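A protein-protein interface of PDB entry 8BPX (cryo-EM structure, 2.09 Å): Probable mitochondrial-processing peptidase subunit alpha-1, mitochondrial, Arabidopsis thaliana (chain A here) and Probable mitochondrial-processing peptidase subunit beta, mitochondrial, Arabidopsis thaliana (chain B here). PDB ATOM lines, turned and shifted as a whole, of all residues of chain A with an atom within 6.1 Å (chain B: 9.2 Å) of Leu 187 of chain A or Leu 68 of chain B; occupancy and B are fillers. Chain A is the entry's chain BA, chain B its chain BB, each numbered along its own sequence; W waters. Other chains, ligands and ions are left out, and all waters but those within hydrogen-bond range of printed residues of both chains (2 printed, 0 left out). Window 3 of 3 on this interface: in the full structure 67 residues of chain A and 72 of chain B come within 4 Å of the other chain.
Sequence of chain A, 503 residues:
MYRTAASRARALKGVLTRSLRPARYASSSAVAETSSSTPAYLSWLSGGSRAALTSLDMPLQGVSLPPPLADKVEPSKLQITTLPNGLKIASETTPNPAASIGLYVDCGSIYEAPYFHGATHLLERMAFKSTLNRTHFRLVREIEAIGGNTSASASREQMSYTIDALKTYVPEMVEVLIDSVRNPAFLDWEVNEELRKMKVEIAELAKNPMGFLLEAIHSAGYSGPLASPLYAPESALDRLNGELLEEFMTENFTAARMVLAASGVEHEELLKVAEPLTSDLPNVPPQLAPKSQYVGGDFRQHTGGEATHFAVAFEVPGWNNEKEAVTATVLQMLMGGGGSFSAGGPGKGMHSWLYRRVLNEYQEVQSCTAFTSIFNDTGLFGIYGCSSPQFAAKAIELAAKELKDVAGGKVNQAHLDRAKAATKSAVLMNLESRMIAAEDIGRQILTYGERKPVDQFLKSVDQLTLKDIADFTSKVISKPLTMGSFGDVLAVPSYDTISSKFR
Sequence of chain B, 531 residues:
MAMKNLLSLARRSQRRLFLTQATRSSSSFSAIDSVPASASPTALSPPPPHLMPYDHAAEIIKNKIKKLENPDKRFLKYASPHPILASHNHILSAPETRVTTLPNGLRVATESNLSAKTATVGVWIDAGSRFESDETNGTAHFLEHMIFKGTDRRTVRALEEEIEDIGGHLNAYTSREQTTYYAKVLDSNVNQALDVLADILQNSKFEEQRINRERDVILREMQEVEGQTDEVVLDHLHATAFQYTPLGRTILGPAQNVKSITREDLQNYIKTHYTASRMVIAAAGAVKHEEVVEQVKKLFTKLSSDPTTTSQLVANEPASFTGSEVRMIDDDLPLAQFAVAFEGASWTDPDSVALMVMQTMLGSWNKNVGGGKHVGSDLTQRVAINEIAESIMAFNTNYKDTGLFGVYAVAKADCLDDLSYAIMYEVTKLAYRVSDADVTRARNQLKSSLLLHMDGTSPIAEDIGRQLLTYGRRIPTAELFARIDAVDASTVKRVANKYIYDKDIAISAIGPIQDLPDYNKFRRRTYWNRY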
ATOM      1  N   MET A 126      -3.920 -20.196  -5.355  1.00  0.00           N
ATOM      2  CA  MET A 126      -2.833 -19.267  -5.639  1.00  0.00           C
ATOM      3  C   MET A 126      -2.349 -18.516  -4.407  1.00  0.00           C
ATOM      4  O   MET A 126      -1.515 -17.616  -4.535  1.00  0.00           O
ATOM      5  CB  MET A 126      -3.257 -18.255  -6.712  1.00  0.00           C
ATOM      6  CG  MET A 126      -3.344 -18.824  -8.115  1.00  0.00           C
ATOM      7  SD  MET A 126      -1.745 -19.260  -8.819  1.00  0.00           S
ATOM      8  CE  MET A 126      -0.774 -17.818  -8.394  1.00  0.00           C
ATOM      9  N   SER A 130       4.069 -16.063  -5.488  1.00  0.00           N
ATOM     10  CA  SER A 130       4.909 -14.886  -5.678  1.00  0.00           C
ATOM     11  C   SER A 130       4.096 -13.602  -5.544  1.00  0.00           C
ATOM     12  O   SER A 130       2.952 -13.521  -5.994  1.00  0.00           O
ATOM     13  CB  SER A 130       5.581 -14.925  -7.052  1.00  0.00           C
ATOM     14  OG  SER A 130       6.288 -16.131  -7.264  1.00  0.00           O
ATOM     15  N   THR A 131       4.695 -12.599  -4.916  1.00  0.00           N
ATOM     16  CA  THR A 131       4.137 -11.259  -4.837  1.00  0.00           C
ATOM     17  C   THR A 131       5.005 -10.299  -5.644  1.00  0.00           C
ATOM     18  O   THR A 131       6.031 -10.677  -6.215  1.00  0.00           O
ATOM     19  CB  THR A 131       4.018 -10.784  -3.384  1.00  0.00           C
ATOM     20  OG1 THR A 131       5.317 -10.499  -2.855  1.00  0.00           O
ATOM     21  CG2 THR A 131       3.336 -11.834  -2.521  1.00  0.00           C
ATOM     22  N   LEU A 132       4.585  -9.036  -5.679  1.00  0.00           N
ATOM     23  CA  LEU A 132       5.375  -8.009  -6.346  1.00  0.00           C
ATOM     24  C   LEU A 132       6.667  -7.700  -5.601  1.00  0.00           C
ATOM     25  O   LEU A 132       7.553  -7.059  -6.168  1.00  0.00           O
ATOM     26  CB  LEU A 132       4.545  -6.734  -6.512  1.00  0.00           C
ATOM     27  CG  LEU A 132       3.195  -6.893  -7.219  1.00  0.00           C
ATOM     28  CD1 LEU A 132       2.398  -5.599  -7.167  1.00  0.00           C
ATOM     29  CD2 LEU A 132       3.376  -7.357  -8.658  1.00  0.00           C
ATOM     30  N   ASN A 133       6.800  -8.151  -4.352  1.00  0.00           N
ATOM     31  CA  ASN A 133       7.963  -7.833  -3.538  1.00  0.00           C
ATOM     32  C   ASN A 133       8.846  -9.029  -3.212  1.00  0.00           C
ATOM     33  O   ASN A 133       9.982  -8.829  -2.776  1.00  0.00           O
ATOM     34  CB  ASN A 133       7.520  -7.169  -2.229  1.00  0.00           C
ATOM     35  CG  ASN A 133       6.689  -5.928  -2.469  1.00  0.00           C
ATOM     36  OD1 ASN A 133       7.148  -4.982  -3.106  1.00  0.00           O
ATOM     37  ND2 ASN A 133       5.456  -5.933  -1.984  1.00  0.00           N
ATOM     38  N   ALA A 185       1.399 -11.389  -7.520  1.00  0.00           N
ATOM     39  CA  ALA A 185       1.952 -11.152  -8.844  1.00  0.00           C
ATOM     40  C   ALA A 185       1.124 -11.825  -9.931  1.00  0.00           C
ATOM     41  O   ALA A 185       1.074 -11.326 -11.059  1.00  0.00           O
ATOM     42  CB  ALA A 185       3.402 -11.631  -8.896  1.00  0.00           C
ATOM     43  N   PHE A 186       0.462 -12.935  -9.602  1.00  0.00           N
ATOM     44  CA  PHE A 186      -0.318 -13.726 -10.555  1.00  0.00           C
ATOM     45  C   PHE A 186       0.470 -13.998 -11.835  1.00  0.00           C
ATOM     46  O   PHE A 186      -0.006 -13.780 -12.950  1.00  0.00           O
ATOM     47  CB  PHE A 186      -1.660 -13.056 -10.862  1.00  0.00           C
ATOM     48  CG  PHE A 186      -2.607 -13.046  -9.698  1.00  0.00           C
ATOM     49  CD1 PHE A 186      -2.817 -14.193  -8.948  1.00  0.00           C
ATOM     50  CD2 PHE A 186      -3.286 -11.894  -9.351  1.00  0.00           C
ATOM     51  CE1 PHE A 186      -3.681 -14.188  -7.874  1.00  0.00           C
ATOM     52  CE2 PHE A 186      -4.155 -11.882  -8.278  1.00  0.00           C
ATOM     53  CZ  PHE A 186      -4.352 -13.029  -7.537  1.00  0.00           C
ATOM     54  N   LEU A 187       1.698 -14.484 -11.661  1.00  0.00           N
ATOM     55  CA  LEU A 187       2.534 -14.838 -12.799  1.00  0.00           C
ATOM     56  C   LEU A 187       1.907 -15.987 -13.577  1.00  0.00           C
ATOM     57  O   LEU A 187       1.327 -16.910 -12.997  1.00  0.00           O
ATOM     58  CB  LEU A 187       3.938 -15.219 -12.332  1.00  0.00           C
ATOM     59  CG  LEU A 187       4.624 -14.266 -11.356  1.00  0.00           C
ATOM     60  CD1 LEU A 187       5.920 -14.869 -10.842  1.00  0.00           C
ATOM     61  CD2 LEU A 187       4.864 -12.900 -11.996  1.00  0.00           C
ATOM     62  N   ASP A 188       2.037 -15.931 -14.903  1.00  0.00           N
ATOM     63  CA  ASP A 188       1.302 -16.854 -15.763  1.00  0.00           C
ATOM     64  C   ASP A 188       1.733 -18.301 -15.556  1.00  0.00           C
ATOM     65  O   ASP A 188       0.896 -19.208 -15.582  1.00  0.00           O
ATOM     66  CB  ASP A 188       1.462 -16.447 -17.224  1.00  0.00           C
ATOM     67  CG  ASP A 188       0.659 -15.218 -17.571  1.00  0.00           C
ATOM     68  OD1 ASP A 188      -0.550 -15.191 -17.258  1.00  0.00           O
ATOM     69  OD2 ASP A 188       1.233 -14.273 -18.152  1.00  0.00           O
ATOM     70  N   TRP A 189       3.033 -18.549 -15.373  1.00  0.00           N
ATOM     71  CA  TRP A 189       3.481 -19.929 -15.197  1.00  0.00           C
ATOM     72  C   TRP A 189       2.977 -20.514 -13.878  1.00  0.00           C
ATOM     73  O   TRP A 189       2.571 -21.683 -13.826  1.00  0.00           O
ATOM     74  CB  TRP A 189       5.010 -20.024 -15.301  1.00  0.00           C
ATOM     75  CG  TRP A 189       5.798 -18.925 -14.636  1.00  0.00           C
ATOM     76  CD1 TRP A 189       6.457 -19.001 -13.446  1.00  0.00           C
ATOM     77  CD2 TRP A 189       6.044 -17.605 -15.144  1.00  0.00           C
ATOM     78  NE1 TRP A 189       7.081 -17.811 -13.171  1.00  0.00           N
ATOM     79  CE2 TRP A 189       6.844 -16.937 -14.196  1.00  0.00           C
ATOM     80  CE3 TRP A 189       5.659 -16.923 -16.300  1.00  0.00           C
ATOM     81  CZ2 TRP A 189       7.266 -15.622 -14.371  1.00  0.00           C
ATOM     82  CZ3 TRP A 189       6.078 -15.616 -16.469  1.00  0.00           C
ATOM     83  CH2 TRP A 189       6.873 -14.980 -15.510  1.00  0.00           C
ATOM     84  N   GLU A 190       2.966 -19.710 -12.815  1.00  0.00           N
ATOM     85  CA  GLU A 190       2.431 -20.170 -11.535  1.00  0.00           C
ATOM     86  C   GLU A 190       0.933 -20.454 -11.635  1.00  0.00           C
ATOM     87  O   GLU A 190       0.440 -21.465 -11.115  1.00  0.00           O
ATOM     88  CB  GLU A 190       2.729 -19.128 -10.452  1.00  0.00           C
ATOM     89  CG  GLU A 190       4.222 -18.939 -10.192  1.00  0.00           C
ATOM     90  CD  GLU A 190       4.533 -18.098  -8.963  1.00  0.00           C
ATOM     91  OE1 GLU A 190       3.597 -17.591  -8.317  1.00  0.00           O
ATOM     92  OE2 GLU A 190       5.729 -17.930  -8.650  1.00  0.00           O
ATOM     93  N   VAL A 191       0.196 -19.573 -12.318  1.00  0.00           N
ATOM     94  CA  VAL A 191      -1.238 -19.780 -12.514  1.00  0.00           C
ATOM     95  C   VAL A 191      -1.492 -21.048 -13.322  1.00  0.00           C
ATOM     96  O   VAL A 191      -2.406 -21.821 -13.021  1.00  0.00           O
ATOM     97  CB  VAL A 191      -1.878 -18.547 -13.175  1.00  0.00           C
ATOM     98  CG1 VAL A 191      -3.342 -18.808 -13.482  1.00  0.00           C
ATOM     99  CG2 VAL A 191      -1.758 -17.340 -12.270  1.00  0.00           C
ATOM    100  N   ASN A 192      -0.698 -21.272 -14.371  1.00  0.00           N
ATOM    101  CA  ASN A 192      -0.875 -22.471 -15.187  1.00  0.00           C
ATOM    102  C   ASN A 192      -0.595 -23.733 -14.380  1.00  0.00           C
ATOM    103  O   ASN A 192      -1.296 -24.742 -14.527  1.00  0.00           O
ATOM    104  CB  ASN A 192       0.025 -22.410 -16.421  1.00  0.00           C
ATOM    105  CG  ASN A 192      -0.417 -21.355 -17.415  1.00  0.00           C
ATOM    106  OD1 ASN A 192      -1.518 -20.816 -17.321  1.00  0.00           O
ATOM    107  ND2 ASN A 192       0.444 -21.058 -18.381  1.00  0.00           N
ATOM    108  N   GLY A 242      -4.162 -15.021 -15.222  1.00  0.00           N
ATOM    109  CA  GLY A 242      -3.731 -14.117 -14.139  1.00  0.00           C
ATOM    110  C   GLY A 242      -4.368 -12.761 -14.140  1.00  0.00           C
ATOM    111  O   GLY A 242      -4.485 -12.160 -13.106  1.00  0.00           O
ATOM    112  N   ILE B  61       4.110  -8.603 -21.470  1.00  0.00           N
ATOM    113  CA  ILE B  61       4.918  -9.414 -20.561  1.00  0.00           C
ATOM    114  C   ILE B  61       6.158  -8.646 -20.103  1.00  0.00           C
ATOM    115  O   ILE B  61       6.594  -8.795 -18.955  1.00  0.00           O
ATOM    116  CB  ILE B  61       5.267 -10.777 -21.197  1.00  0.00           C
ATOM    117  CG1 ILE B  61       5.752 -11.766 -20.132  1.00  0.00           C
ATOM    118  CG2 ILE B  61       6.314 -10.644 -22.287  1.00  0.00           C
ATOM    119  CD1 ILE B  61       4.854 -11.874 -18.924  1.00  0.00           C
ATOM    120  N   LYS B  62       6.731  -7.800 -20.967  1.00  0.00           N
ATOM    121  CA  LYS B  62       7.889  -7.006 -20.571  1.00  0.00           C
ATOM    122  C   LYS B  62       7.531  -6.008 -19.472  1.00  0.00           C
ATOM    123  O   LYS B  62       8.289  -5.840 -18.510  1.00  0.00           O
ATOM    124  CB  LYS B  62       8.468  -6.283 -21.787  1.00  0.00           C
ATOM    125  CG  LYS B  62       9.422  -7.122 -22.622  1.00  0.00           C
ATOM    126  CD  LYS B  62      10.145  -6.272 -23.657  1.00  0.00           C
ATOM    127  CE  LYS B  62       9.238  -5.918 -24.820  1.00  0.00           C
ATOM    128  NZ  LYS B  62       9.984  -5.273 -25.931  1.00  0.00           N
ATOM    129  N   ASN B  63       6.383  -5.339 -19.595  1.00  0.00           N
ATOM    130  CA  ASN B  63       5.955  -4.419 -18.543  1.00  0.00           C
ATOM    131  C   ASN B  63       5.698  -5.160 -17.234  1.00  0.00           C
ATOM    132  O   ASN B  63       6.087  -4.693 -16.152  1.00  0.00           O
ATOM    133  CB  ASN B  63       4.706  -3.659 -18.985  1.00  0.00           C
ATOM    134  CG  ASN B  63       4.970  -2.755 -20.165  1.00  0.00           C
ATOM    135  OD1 ASN B  63       5.999  -2.085 -20.229  1.00  0.00           O
ATOM    136  ND2 ASN B  63       4.045  -2.737 -21.115  1.00  0.00           N
ATOM    137  N   LYS B  64       5.063  -6.332 -17.317  1.00  0.00           N
ATOM    138  CA  LYS B  64       4.845  -7.126 -16.111  1.00  0.00           C
ATOM    139  C   LYS B  64       6.164  -7.499 -15.447  1.00  0.00           C
ATOM    140  O   LYS B  64       6.298  -7.401 -14.222  1.00  0.00           O
ATOM    141  CB  LYS B  64       4.040  -8.377 -16.443  1.00  0.00           C
ATOM    142  CG  LYS B  64       2.827  -8.549 -15.569  1.00  0.00           C
ATOM    143  CD  LYS B  64       3.237  -8.941 -14.165  1.00  0.00           C
ATOM    144  CE  LYS B  64       2.037  -9.332 -13.335  1.00  0.00           C
ATOM    145  NZ  LYS B  64       2.309  -9.173 -11.882  1.00  0.00           N
ATOM    146  N   ILE B  65       7.151  -7.923 -16.238  1.00  0.00           N
ATOM    147  CA  ILE B  65       8.475  -8.214 -15.696  1.00  0.00           C
ATOM    148  C   ILE B  65       9.055  -6.974 -15.033  1.00  0.00           C
ATOM    149  O   ILE B  65       9.659  -7.049 -13.955  1.00  0.00           O
ATOM    150  CB  ILE B  65       9.405  -8.739 -16.806  1.00  0.00           C
ATOM    151  CG1 ILE B  65       9.126 -10.207 -17.110  1.00  0.00           C
ATOM    152  CG2 ILE B  65      10.865  -8.562 -16.423  1.00  0.00           C
ATOM    153  CD1 ILE B  65       9.789 -10.664 -18.377  1.00  0.00           C
ATOM    154  N   LYS B  66       8.874  -5.814 -15.666  1.00  0.00           N
ATOM    155  CA  LYS B  66       9.447  -4.579 -15.143  1.00  0.00           C
ATOM    156  C   LYS B  66       8.903  -4.266 -13.757  1.00  0.00           C
ATOM    157  O   LYS B  66       9.653  -3.831 -12.877  1.00  0.00           O
ATOM    158  CB  LYS B  66       9.191  -3.429 -16.128  1.00  0.00           C
ATOM    159  CG  LYS B  66       9.901  -3.492 -17.491  1.00  0.00           C
ATOM    160  CD  LYS B  66       9.583  -2.327 -18.433  1.00  0.00           C
ATOM    161  CE  LYS B  66      10.340  -2.446 -19.746  1.00  0.00           C
ATOM    162  NZ  LYS B  66      10.030  -1.338 -20.689  1.00  0.00           N
ATOM    163  N   LYS B  67       7.604  -4.482 -13.536  1.00  0.00           N
ATOM    164  CA  LYS B  67       7.117  -4.125 -12.204  1.00  0.00           C
ATOM    165  C   LYS B  67       7.469  -5.152 -11.128  1.00  0.00           C
ATOM    166  O   LYS B  67       6.895  -5.086 -10.037  1.00  0.00           O
ATOM    167  CB  LYS B  67       5.605  -3.891 -12.205  1.00  0.00           C
ATOM    168  CG  LYS B  67       4.772  -5.048 -12.686  1.00  0.00           C
ATOM    169  CD  LYS B  67       3.298  -4.719 -12.570  1.00  0.00           C
ATOM    170  CE  LYS B  67       2.759  -4.126 -13.858  1.00  0.00           C
ATOM    171  NZ  LYS B  67       2.531  -5.161 -14.902  1.00  0.00           N
ATOM    172  N   LEU B  68       8.370  -6.097 -11.394  1.00  0.00           N
ATOM    173  CA  LEU B  68       8.919  -6.956 -10.353  1.00  0.00           C
ATOM    174  C   LEU B  68      10.338  -6.568  -9.963  1.00  0.00           C
ATOM    175  O   LEU B  68      10.913  -7.190  -9.066  1.00  0.00           O
ATOM    176  CB  LEU B  68       8.895  -8.422 -10.796  1.00  0.00           C
ATOM    177  CG  LEU B  68       7.538  -9.051 -11.117  1.00  0.00           C
ATOM    178  CD1 LEU B  68       7.725 -10.313 -11.948  1.00  0.00           C
ATOM    179  CD2 LEU B  68       6.758  -9.347  -9.844  1.00  0.00           C
ATOM    180  N   GLU B  69      10.911  -5.554 -10.606  1.00  0.00           N
ATOM    181  CA  GLU B  69      12.283  -5.148 -10.353  1.00  0.00           C
ATOM    182  C   GLU B  69      12.409  -4.088  -9.266  1.00  0.00           C
ATOM    183  O   GLU B  69      13.524  -3.837  -8.800  1.00  0.00           O
ATOM    184  CB  GLU B  69      12.920  -4.630 -11.646  1.00  0.00           C
ATOM    185  CG  GLU B  69      13.225  -5.718 -12.661  1.00  0.00           C
ATOM    186  CD  GLU B  69      14.682  -6.117 -12.668  1.00  0.00           C
ATOM    187  OE1 GLU B  69      15.294  -6.113 -13.755  1.00  0.00           O
ATOM    188  OE2 GLU B  69      15.218  -6.441 -11.587  1.00  0.00           O
ATOM    189  N   ASN B  70      11.307  -3.465  -8.852  1.00  0.00           N
ATOM    190  CA  ASN B  70      11.317  -2.439  -7.809  1.00  0.00           C
ATOM    191  C   ASN B  70      10.311  -2.810  -6.728  1.00  0.00           C
ATOM    192  O   ASN B  70       9.165  -2.339  -6.738  1.00  0.00           O
ATOM    193  CB  ASN B  70      11.024  -1.054  -8.387  1.00  0.00           C
ATOM    194  CG  ASN B  70      11.650  -0.850  -9.752  1.00  0.00           C
ATOM    195  OD1 ASN B  70      10.958  -0.560 -10.728  1.00  0.00           O
ATOM    196  ND2 ASN B  70      12.965  -1.002  -9.829  1.00  0.00           N
ATOM    197  N   PRO B  71      10.701  -3.661  -5.783  1.00  0.00           N
ATOM    198  CA  PRO B  71       9.807  -3.983  -4.668  1.00  0.00           C
ATOM    199  C   PRO B  71       9.645  -2.813  -3.711  1.00  0.00           C
ATOM    200  O   PRO B  71      10.539  -1.980  -3.549  1.00  0.00           O
ATOM    201  CB  PRO B  71      10.508  -5.161  -3.984  1.00  0.00           C
ATOM    202  CG  PRO B  71      11.941  -4.984  -4.334  1.00  0.00           C
ATOM    203  CD  PRO B  71      11.959  -4.423  -5.721  1.00  0.00           C
ATOM    204  N   ASP B  72       8.482  -2.766  -3.064  1.00  0.00           N
ATOM    205  CA  ASP B  72       8.212  -1.773  -2.032  1.00  0.00           C
ATOM    206  C   ASP B  72       8.824  -2.235  -0.713  1.00  0.00           C
ATOM    207  O   ASP B  72       8.433  -3.274  -0.171  1.00  0.00           O
ATOM    208  CB  ASP B  72       6.707  -1.554  -1.888  1.00  0.00           C
ATOM    209  CG  ASP B  72       6.358  -0.602  -0.760  1.00  0.00           C
ATOM    210  OD1 ASP B  72       7.227   0.197  -0.355  1.00  0.00           O
ATOM    211  OD2 ASP B  72       5.207  -0.648  -0.281  1.00  0.00           O
ATOM    212  N   LEU B  76       9.378  -5.500   3.248  1.00  0.00           N
ATOM    213  CA  LEU B  76      10.613  -6.280   3.260  1.00  0.00           C
ATOM    214  C   LEU B  76      11.515  -5.846   4.409  1.00  0.00           C
ATOM    215  O   LEU B  76      12.715  -5.632   4.241  1.00  0.00           O
ATOM    216  CB  LEU B  76      11.352  -6.154   1.926  1.00  0.00           C
ATOM    217  CG  LEU B  76      10.727  -6.801   0.688  1.00  0.00           C
ATOM    218  CD1 LEU B  76      11.630  -6.622  -0.518  1.00  0.00           C
ATOM    219  CD2 LEU B  76      10.439  -8.269   0.921  1.00  0.00           C
HETATM  220  O   HOH W   1       9.819  -8.315  -6.702  1.00  0.00           O
HETATM  221  O   HOH W   2       6.179  -3.581  -5.446  1.00  0.00           O
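Hydrophobic or aromatic side chains of chain A within 4 Å of the printed part of chain B: Leu 132 and Leu 187. Along chain A the printed residues that touch a printed residue of chain B span positions 131 to 187. Printed residues of chain B that touch a printed residue of chain A: Lys 64, Leu 68, Pro 71, Asp 72 and Leu 76. Hydrophobic or aromatic side chains of chain B within 4 Å of the printed part of chain A: Leu 68, Pro 71 and Leu 76. Among the printed residues, 8 pairs touch across the chains.
Leu 68 of chain B touches Thr 131 of chain A. Lys 64 of chain B touches Leu 132 of chain A (NZ to CD2, 3.9 Å). Leu 132 of chain A touches Leu 68 of chain B (CA to CD2, 3.99 Å). Asn 133 of chain A touches Pro 71 of chain B (OD1 to CA, 3.2 Å). Asn 133 of chain A touches Leu 76 of chain B (O to CD1, 3.6 Å). Leu 68 of chain B touches Leu 187 of chain A.
Of the printed residues of chain A, Leu 68 of chain B touches Thr 131, Leu 132 and Leu 187. Of the printed residues of chain B, Leu 132 of chain A touches Lys 64 (3.9 Å) and Leu 68 (3.99 Å). Printed residues of chain A within 4 Å of Pro 71 of chain B: Asn 133 (3.2 Å). The nearest printed residue of chain A that does not touch Leu 68 of chain B is Ala 185 of chain A (4.2 Å).
The backbone carbonyl oxygen (O) of Ala 185 of chain A sits at hydrogen-bond distance from the side-chain amino group (NZ) of Lys 64 of chain B, at 2.6 Å. OD1 of Asn 133 of chain A sits at hydrogen-bond distance from N of Asp 72 of chain B (2.6 Å).
OG1 of Thr 131 of chain A lies close to N of Asn 133 of chain A. The backbone NH of Ala 185 of chain A is in hydrogen-bond range of the backbone carbonyl oxygen of Ser 130 of chain A (3.0 Å).
Water W1 lies within hydrogen-bond range of O of Leu 132 of chain A and O of Leu 68 of chain B. Water W2 lies within hydrogen-bond range of the side-chain amide oxygen (OD1) of Asn 133 of chain A, the backbone NH (N) of Asp 72 of chain B and the backbone carbonyl oxygen (O) of Asn 70 of chain B.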
